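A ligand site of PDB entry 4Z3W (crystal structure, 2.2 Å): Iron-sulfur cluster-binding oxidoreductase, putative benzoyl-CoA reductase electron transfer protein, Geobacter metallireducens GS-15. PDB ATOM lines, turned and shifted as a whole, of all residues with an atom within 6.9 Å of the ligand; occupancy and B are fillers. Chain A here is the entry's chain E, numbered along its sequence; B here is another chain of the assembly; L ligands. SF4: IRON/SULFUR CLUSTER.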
ATOM      1  N   ILE A  15      -7.916  -0.690  21.787  1.00  0.00           N
ATOM      2  CA  ILE A  15      -8.665   0.551  21.665  1.00  0.00           C
ATOM      3  C   ILE A  15      -7.880   1.732  22.207  1.00  0.00           C
ATOM      4  O   ILE A  15      -7.677   1.846  23.423  1.00  0.00           O
ATOM      5  CB  ILE A  15     -10.011   0.462  22.410  1.00  0.00           C
ATOM      6  CG1 ILE A  15     -10.777  -0.792  22.011  1.00  0.00           C
ATOM      7  CG2 ILE A  15     -10.830   1.711  22.182  1.00  0.00           C
ATOM      8  CD1 ILE A  15     -11.950  -1.102  22.927  1.00  0.00           C
ATOM      9  N   LYS A  19      -6.922   8.396  20.473  1.00  0.00           N
ATOM     10  CA  LYS A  19      -6.974   8.728  19.047  1.00  0.00           C
ATOM     11  C   LYS A  19      -8.403   8.834  18.515  1.00  0.00           C
ATOM     12  O   LYS A  19      -8.594   9.151  17.352  1.00  0.00           O
ATOM     13  CB  LYS A  19      -6.244   7.683  18.197  1.00  0.00           C
ATOM     14  CG  LYS A  19      -4.728   7.739  18.204  1.00  0.00           C
ATOM     15  CD  LYS A  19      -4.227   6.709  17.198  1.00  0.00           C
ATOM     16  CE  LYS A  19      -2.748   6.418  17.323  1.00  0.00           C
ATOM     17  NZ  LYS A  19      -2.335   5.501  16.206  1.00  0.00           N
ATOM     18  N   CYS A  20      -9.402   8.534  19.336  1.00  0.00           N
ATOM     19  CA  CYS A  20     -10.752   8.495  18.820  1.00  0.00           C
ATOM     20  C   CYS A  20     -11.284   9.909  18.639  1.00  0.00           C
ATOM     21  O   CYS A  20     -11.023  10.800  19.443  1.00  0.00           O
ATOM     22  CB  CYS A  20     -11.670   7.699  19.734  1.00  0.00           C
ATOM     23  SG  CYS A  20     -13.364   7.607  19.137  1.00  0.00           S
ATOM     24  N   ASN A  21     -12.058  10.117  17.585  1.00  0.00           N
ATOM     25  CA  ASN A  21     -12.516  11.466  17.284  1.00  0.00           C
ATOM     26  C   ASN A  21     -14.035  11.588  17.369  1.00  0.00           C
ATOM     27  O   ASN A  21     -14.576  12.651  17.143  1.00  0.00           O
ATOM     28  CB  ASN A  21     -12.010  11.940  15.914  1.00  0.00           C
ATOM     29  CG  ASN A  21     -12.471  11.062  14.758  1.00  0.00           C
ATOM     30  OD1 ASN A  21     -13.648  10.706  14.653  1.00  0.00           O
ATOM     31  ND2 ASN A  21     -11.550  10.699  13.879  1.00  0.00           N
ATOM     32  N   GLY A  22     -14.704  10.493  17.740  1.00  0.00           N
ATOM     33  CA  GLY A  22     -16.110  10.530  18.089  1.00  0.00           C
ATOM     34  C   GLY A  22     -17.080  10.432  16.929  1.00  0.00           C
ATOM     35  O   GLY A  22     -18.287  10.590  17.103  1.00  0.00           O
ATOM     36  N   CYS A  23     -16.549  10.130  15.742  1.00  0.00           N
ATOM     37  CA  CYS A  23     -17.315  10.157  14.500  1.00  0.00           C
ATOM     38  C   CYS A  23     -18.311   9.020  14.422  1.00  0.00           C
ATOM     39  O   CYS A  23     -19.251   9.065  13.643  1.00  0.00           O
ATOM     40  CB  CYS A  23     -16.364  10.083  13.311  1.00  0.00           C
ATOM     41  SG  CYS A  23     -15.548   8.490  13.057  1.00  0.00           S
ATOM     42  N   ARG A  24     -18.102   7.983  15.215  1.00  0.00           N
ATOM     43  CA  ARG A  24     -19.045   6.861  15.249  1.00  0.00           C
ATOM     44  C   ARG A  24     -19.191   6.159  13.895  1.00  0.00           C
ATOM     45  O   ARG A  24     -20.192   5.491  13.639  1.00  0.00           O
ATOM     46  CB  ARG A  24     -20.437   7.334  15.733  1.00  0.00           C
ATOM     47  CG  ARG A  24     -20.436   7.965  17.128  1.00  0.00           C
ATOM     48  CD  ARG A  24     -21.768   8.619  17.470  1.00  0.00           C
ATOM     49  NE  ARG A  24     -22.888   7.800  17.011  1.00  0.00           N
ATOM     50  CZ  ARG A  24     -24.105   8.282  16.754  1.00  0.00           C
ATOM     51  NH1 ARG A  24     -24.360   9.580  16.915  1.00  0.00           N
ATOM     52  NH2 ARG A  24     -25.059   7.465  16.325  1.00  0.00           N
ATOM     53  N   ALA A  25     -18.177   6.278  13.031  1.00  0.00           N
ATOM     54  CA  ALA A  25     -18.133   5.529  11.779  1.00  0.00           C
ATOM     55  C   ALA A  25     -18.202   4.033  12.024  1.00  0.00           C
ATOM     56  O   ALA A  25     -18.751   3.268  11.215  1.00  0.00           O
ATOM     57  CB  ALA A  25     -16.857   5.886  10.986  1.00  0.00           C
ATOM     58  N   CYS A  26     -17.640   3.610  13.143  1.00  0.00           N
ATOM     59  CA  CYS A  26     -17.609   2.202  13.517  1.00  0.00           C
ATOM     60  C   CYS A  26     -19.009   1.656  13.762  1.00  0.00           C
ATOM     61  O   CYS A  26     -19.329   0.524  13.363  1.00  0.00           O
ATOM     62  CB  CYS A  26     -16.727   2.014  14.764  1.00  0.00           C
ATOM     63  SG  CYS A  26     -16.958   3.279  16.025  1.00  0.00           S
ATOM     64  N   GLU A  27     -19.868   2.441  14.389  1.00  0.00           N
ATOM     65  CA  GLU A  27     -21.245   2.003  14.628  1.00  0.00           C
ATOM     66  C   GLU A  27     -22.011   1.883  13.309  1.00  0.00           C
ATOM     67  O   GLU A  27     -22.859   1.002  13.147  1.00  0.00           O
ATOM     68  CB  GLU A  27     -21.978   2.952  15.552  1.00  0.00           C
ATOM     69  CG  GLU A  27     -21.250   3.327  16.793  1.00  0.00           C
ATOM     70  CD  GLU A  27     -22.093   4.193  17.705  1.00  0.00           C
ATOM     71  OE1 GLU A  27     -23.169   4.644  17.253  1.00  0.00           O
ATOM     72  OE2 GLU A  27     -21.690   4.431  18.861  1.00  0.00           O
ATOM     73  N   VAL A  49     -20.353  -2.383  18.394  1.00  0.00           N
ATOM     74  CA  VAL A  49     -19.445  -1.429  19.005  1.00  0.00           C
ATOM     75  C   VAL A  49     -20.249  -0.138  19.193  1.00  0.00           C
ATOM     76  O   VAL A  49     -20.922   0.321  18.263  1.00  0.00           O
ATOM     77  CB  VAL A  49     -18.182  -1.177  18.142  1.00  0.00           C
ATOM     78  CG1 VAL A  49     -18.578  -0.781  16.729  1.00  0.00           C
ATOM     79  CG2 VAL A  49     -17.288  -0.109  18.759  1.00  0.00           C
ATOM     80  N   VAL A  51     -19.902   3.829  20.878  1.00  0.00           N
ATOM     81  CA  VAL A  51     -18.950   4.791  21.416  1.00  0.00           C
ATOM     82  C   VAL A  51     -19.535   5.601  22.567  1.00  0.00           C
ATOM     83  O   VAL A  51     -20.605   6.164  22.426  1.00  0.00           O
ATOM     84  CB  VAL A  51     -18.452   5.755  20.338  1.00  0.00           C
ATOM     85  CG1 VAL A  51     -17.342   6.621  20.888  1.00  0.00           C
ATOM     86  CG2 VAL A  51     -17.971   4.986  19.126  1.00  0.00           C
ATOM     87  N   TYR A  60     -14.197   9.914  24.797  1.00  0.00           N
ATOM     88  CA  TYR A  60     -14.532   9.162  23.580  1.00  0.00           C
ATOM     89  C   TYR A  60     -13.990   7.768  23.750  1.00  0.00           C
ATOM     90  O   TYR A  60     -12.795   7.528  23.612  1.00  0.00           O
ATOM     91  CB  TYR A  60     -13.930   9.807  22.317  1.00  0.00           C
ATOM     92  CG  TYR A  60     -14.149  11.296  22.249  1.00  0.00           C
ATOM     93  CD1 TYR A  60     -13.381  12.151  23.011  1.00  0.00           C
ATOM     94  CD2 TYR A  60     -15.118  11.836  21.416  1.00  0.00           C
ATOM     95  CE1 TYR A  60     -13.590  13.526  22.960  1.00  0.00           C
ATOM     96  CE2 TYR A  60     -15.331  13.223  21.346  1.00  0.00           C
ATOM     97  CZ  TYR A  60     -14.562  14.047  22.125  1.00  0.00           C
ATOM     98  OH  TYR A  60     -14.738  15.395  22.093  1.00  0.00           O
ATOM     99  N   PRO A  62     -14.708   3.841  22.675  1.00  0.00           N
ATOM    100  CA  PRO A  62     -15.434   2.761  21.993  1.00  0.00           C
ATOM    101  C   PRO A  62     -15.599   1.533  22.894  1.00  0.00           C
ATOM    102  O   PRO A  62     -14.637   1.011  23.462  1.00  0.00           O
ATOM    103  CB  PRO A  62     -14.552   2.456  20.787  1.00  0.00           C
ATOM    104  CG  PRO A  62     -13.700   3.722  20.615  1.00  0.00           C
ATOM    105  CD  PRO A  62     -13.432   4.148  22.023  1.00  0.00           C
ATOM    106  N   TYR A  64     -17.048  -2.418  23.211  1.00  0.00           N
ATOM    107  CA  TYR A  64     -17.433  -3.607  22.450  1.00  0.00           C
ATOM    108  C   TYR A  64     -18.422  -4.495  23.227  1.00  0.00           C
ATOM    109  O   TYR A  64     -18.288  -4.694  24.428  1.00  0.00           O
ATOM    110  CB  TYR A  64     -16.193  -4.395  22.035  1.00  0.00           C
ATOM    111  CG  TYR A  64     -15.472  -3.754  20.866  1.00  0.00           C
ATOM    112  CD1 TYR A  64     -14.813  -2.538  21.008  1.00  0.00           C
ATOM    113  CD2 TYR A  64     -15.480  -4.343  19.612  1.00  0.00           C
ATOM    114  CE1 TYR A  64     -14.174  -1.932  19.940  1.00  0.00           C
ATOM    115  CE2 TYR A  64     -14.854  -3.744  18.536  1.00  0.00           C
ATOM    116  CZ  TYR A  64     -14.199  -2.539  18.709  1.00  0.00           C
ATOM    117  OH  TYR A  64     -13.563  -1.953  17.639  1.00  0.00           O
ATOM    118  N   CYS A 124     -15.241  -2.374  11.666  1.00  0.00           N
ATOM    119  CA  CYS A 124     -14.973  -1.212  12.507  1.00  0.00           C
ATOM    120  C   CYS A 124     -13.496  -0.779  12.407  1.00  0.00           C
ATOM    121  O   CYS A 124     -13.200   0.411  12.267  1.00  0.00           O
ATOM    122  CB  CYS A 124     -15.344  -1.490  13.966  1.00  0.00           C
ATOM    123  SG  CYS A 124     -14.576  -2.959  14.765  1.00  0.00           S
ATOM    124  N   TRP A 127     -12.880   0.888   8.921  1.00  0.00           N
ATOM    125  CA  TRP A 127     -13.421   2.226   8.672  1.00  0.00           C
ATOM    126  C   TRP A 127     -12.882   3.266   9.648  1.00  0.00           C
ATOM    127  O   TRP A 127     -13.200   4.439   9.531  1.00  0.00           O
ATOM    128  CB  TRP A 127     -14.960   2.223   8.708  1.00  0.00           C
ATOM    129  CG  TRP A 127     -15.568   1.814   7.390  1.00  0.00           C
ATOM    130  CD1 TRP A 127     -15.076   0.878   6.531  1.00  0.00           C
ATOM    131  CD2 TRP A 127     -16.750   2.343   6.777  1.00  0.00           C
ATOM    132  NE1 TRP A 127     -15.895   0.783   5.426  1.00  0.00           N
ATOM    133  CE2 TRP A 127     -16.919   1.677   5.546  1.00  0.00           C
ATOM    134  CE3 TRP A 127     -17.703   3.311   7.157  1.00  0.00           C
ATOM    135  CZ2 TRP A 127     -17.988   1.951   4.679  1.00  0.00           C
ATOM    136  CZ3 TRP A 127     -18.762   3.583   6.287  1.00  0.00           C
ATOM    137  CH2 TRP A 127     -18.890   2.900   5.065  1.00  0.00           C
ATOM    138  N   CYS A 128     -12.069   2.854  10.608  1.00  0.00           N
ATOM    139  CA  CYS A 128     -11.484   3.851  11.506  1.00  0.00           C
ATOM    140  C   CYS A 128     -10.231   4.404  10.874  1.00  0.00           C
ATOM    141  O   CYS A 128      -9.121   3.967  11.173  1.00  0.00           O
ATOM    142  CB  CYS A 128     -11.179   3.259  12.881  1.00  0.00           C
ATOM    143  SG  CYS A 128     -10.752   4.525  14.096  1.00  0.00           S
ATOM    144  N   LEU A 129     -10.403   5.371   9.981  1.00  0.00           N
ATOM    145  CA  LEU A 129      -9.263   5.820   9.181  1.00  0.00           C
ATOM    146  C   LEU A 129      -8.152   6.411  10.066  1.00  0.00           C
ATOM    147  O   LEU A 129      -6.997   6.365   9.688  1.00  0.00           O
ATOM    148  CB  LEU A 129      -9.724   6.803   8.106  1.00  0.00           C
ATOM    149  CG  LEU A 129      -9.823   6.136   6.712  1.00  0.00           C
ATOM    150  CD1 LEU A 129     -10.748   4.941   6.734  1.00  0.00           C
ATOM    151  CD2 LEU A 129     -10.232   7.113   5.601  1.00  0.00           C
ATOM    152  N   VAL A 130      -8.487   6.936  11.246  1.00  0.00           N
ATOM    153  CA  VAL A 130      -7.443   7.468  12.110  1.00  0.00           C
ATOM    154  C   VAL A 130      -6.724   6.351  12.897  1.00  0.00           C
ATOM    155  O   VAL A 130      -5.679   6.564  13.510  1.00  0.00           O
ATOM    156  CB  VAL A 130      -8.000   8.538  13.083  1.00  0.00           C
ATOM    157  CG1 VAL A 130      -8.679   9.659  12.286  1.00  0.00           C
ATOM    158  CG2 VAL A 130      -8.992   7.941  14.078  1.00  0.00           C
ATOM    159  N   GLY A 131      -7.272   5.134  12.819  1.00  0.00           N
ATOM    160  CA  GLY A 131      -6.607   3.971  13.355  1.00  0.00           C
ATOM    161  C   GLY A 131      -6.601   3.883  14.871  1.00  0.00           C
ATOM    162  O   GLY A 131      -5.564   3.601  15.476  1.00  0.00           O
ATOM    163  N   ALA A 132      -7.748   4.106  15.494  1.00  0.00           N
ATOM    164  CA  ALA A 132      -7.865   4.011  16.947  1.00  0.00           C
ATOM    165  C   ALA A 132      -8.037   2.559  17.401  1.00  0.00           C
ATOM    166  O   ALA A 132      -8.034   2.260  18.595  1.00  0.00           O
ATOM    167  CB  ALA A 132      -9.034   4.853  17.443  1.00  0.00           C
ATOM    168  N   LEU A 133      -8.188   1.660  16.433  1.00  0.00           N
ATOM    169  CA  LEU A 133      -8.684   0.323  16.682  1.00  0.00           C
ATOM    170  C   LEU A 133      -7.885  -0.718  15.929  1.00  0.00           C
ATOM    171  O   LEU A 133      -7.683  -0.583  14.728  1.00  0.00           O
ATOM    172  CB  LEU A 133     -10.149   0.195  16.250  1.00  0.00           C
ATOM    173  CG  LEU A 133     -11.162   1.227  16.724  1.00  0.00           C
ATOM    174  CD1 LEU A 133     -12.448   1.001  15.965  1.00  0.00           C
ATOM    175  CD2 LEU A 133     -11.396   1.077  18.234  1.00  0.00           C
ATOM    176  N   SER B 298     -14.635  14.915  14.861  1.00  0.00           N
ATOM    177  CA  SER B 298     -15.325  14.842  13.569  1.00  0.00           C
ATOM    178  C   SER B 298     -16.834  15.084  13.664  1.00  0.00           C
ATOM    179  O   SER B 298     -17.393  15.103  14.746  1.00  0.00           O
ATOM    180  CB  SER B 298     -15.082  13.475  12.937  1.00  0.00           C
ATOM    181  OG  SER B 298     -13.719  13.272  12.593  1.00  0.00           O
ATOM    182  N   CYS B 302     -17.261  10.666   9.710  1.00  0.00           N
ATOM    183  CA  CYS B 302     -16.200  11.308   8.941  1.00  0.00           C
ATOM    184  C   CYS B 302     -14.861  11.295   9.671  1.00  0.00           C
ATOM    185  O   CYS B 302     -14.797  11.553  10.876  1.00  0.00           O
ATOM    186  CB  CYS B 302     -16.588  12.749   8.621  1.00  0.00           C
ATOM    187  SG  CYS B 302     -15.407  13.566   7.516  1.00  0.00           S
ATOM    188  N   PRO B 303     -13.770  11.038   8.935  1.00  0.00           N
ATOM    189  CA  PRO B 303     -12.448  10.971   9.592  1.00  0.00           C
ATOM    190  C   PRO B 303     -11.663  12.287   9.608  1.00  0.00           C
ATOM    191  O   PRO B 303     -10.588  12.314  10.194  1.00  0.00           O
ATOM    192  CB  PRO B 303     -11.714   9.935   8.753  1.00  0.00           C
ATOM    193  CG  PRO B 303     -12.260  10.149   7.380  1.00  0.00           C
ATOM    194  CD  PRO B 303     -13.729  10.479   7.578  1.00  0.00           C
HETATM  195 FE1  SF4 L   1     -15.135   4.682  15.927  1.00  0.00          FE
HETATM  196 FE2  SF4 L   1     -12.685   5.306  15.044  1.00  0.00          FE
HETATM  197 FE3  SF4 L   1     -13.610   6.344  17.282  1.00  0.00          FE
HETATM  198 FE4  SF4 L   1     -14.546   7.109  14.739  1.00  0.00          FE
HETATM  199  S1  SF4 L   1     -12.487   7.520  15.628  1.00  0.00           S
HETATM  200  S2  SF4 L   1     -15.770   6.711  16.698  1.00  0.00           S
HETATM  201  S3  SF4 L   1     -14.559   5.077  13.710  1.00  0.00           S
HETATM  202  S4  SF4 L   1     -13.168   4.134  16.968  1.00  0.00           S
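A sulfur (S2) of the ligand sits close to the backbone NH (N) of Cys 23 (3.6 Å).
An iron atom (FE2) of the ligand is bound by the side-chain sulfur of Cys 128 (2.3 Å).
FE1 of the ligand is bound by SG of Cys 26, 2.3 Å away.
SG of Cys 23 is bound to FE4 of the ligand.
The side-chain sulfur (SG) of Cys 20 binds an iron atom (FE3) of the ligand (2.3 Å).
The backbone NH (N) of Asn 21 lies close to a sulfur (S1) of the ligand (3.3 Å).
N of Cys 26 sits close to S3 of the ligand.
A sulfur (S1) of the ligand lies close to the side-chain amide oxygen (OD1) of Asn 21 (3.5 Å).
The backbone NH (N) of Arg 24 sits close to a sulfur (S2) of the ligand (3.0 Å).
N of Ser 298 of chain B sits at hydrogen-bond distance from O of Asn 21 (3.2 Å).
The side-chain sulfur of Cys 23 lies close to the backbone NH of Ala 25, at 3.4 Å.
The backbone NH (N) of Cys 23 lies close to the side-chain amide oxygen (OD1) of Asn 21 (3.2 Å).
The backbone NH (N) of Gly 22 lies close to the side-chain sulfur (SG) of Cys 20, 3.5 Å away.
The side-chain sulfur of Cys 128 lies close to the backbone NH of Ala 132 (3.3 Å).
OE1 of Glu 27 is in salt-bridge range of NE of Arg 24 (3.2 Å).
N of Val 51 lies within hydrogen-bond range of OE2 of Glu 27, at 2.8 Å.
SG of Cys 128 lies close to N of Gly 131, 3.8 Å away.
Merely in contact with the ligand: Leu 133 (3.4 Å), Ala 25 (3.7 Å), Val 51 (3.7 Å), Pro 62 (3.7 Å), Val 130 (3.8 Å) and Gly 22 (3.95 Å).
Hydrophobic or aromatic side chains within 4 Å of the ligand: Ala 25, Val 51, Pro 62, Val 130 and Leu 133.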
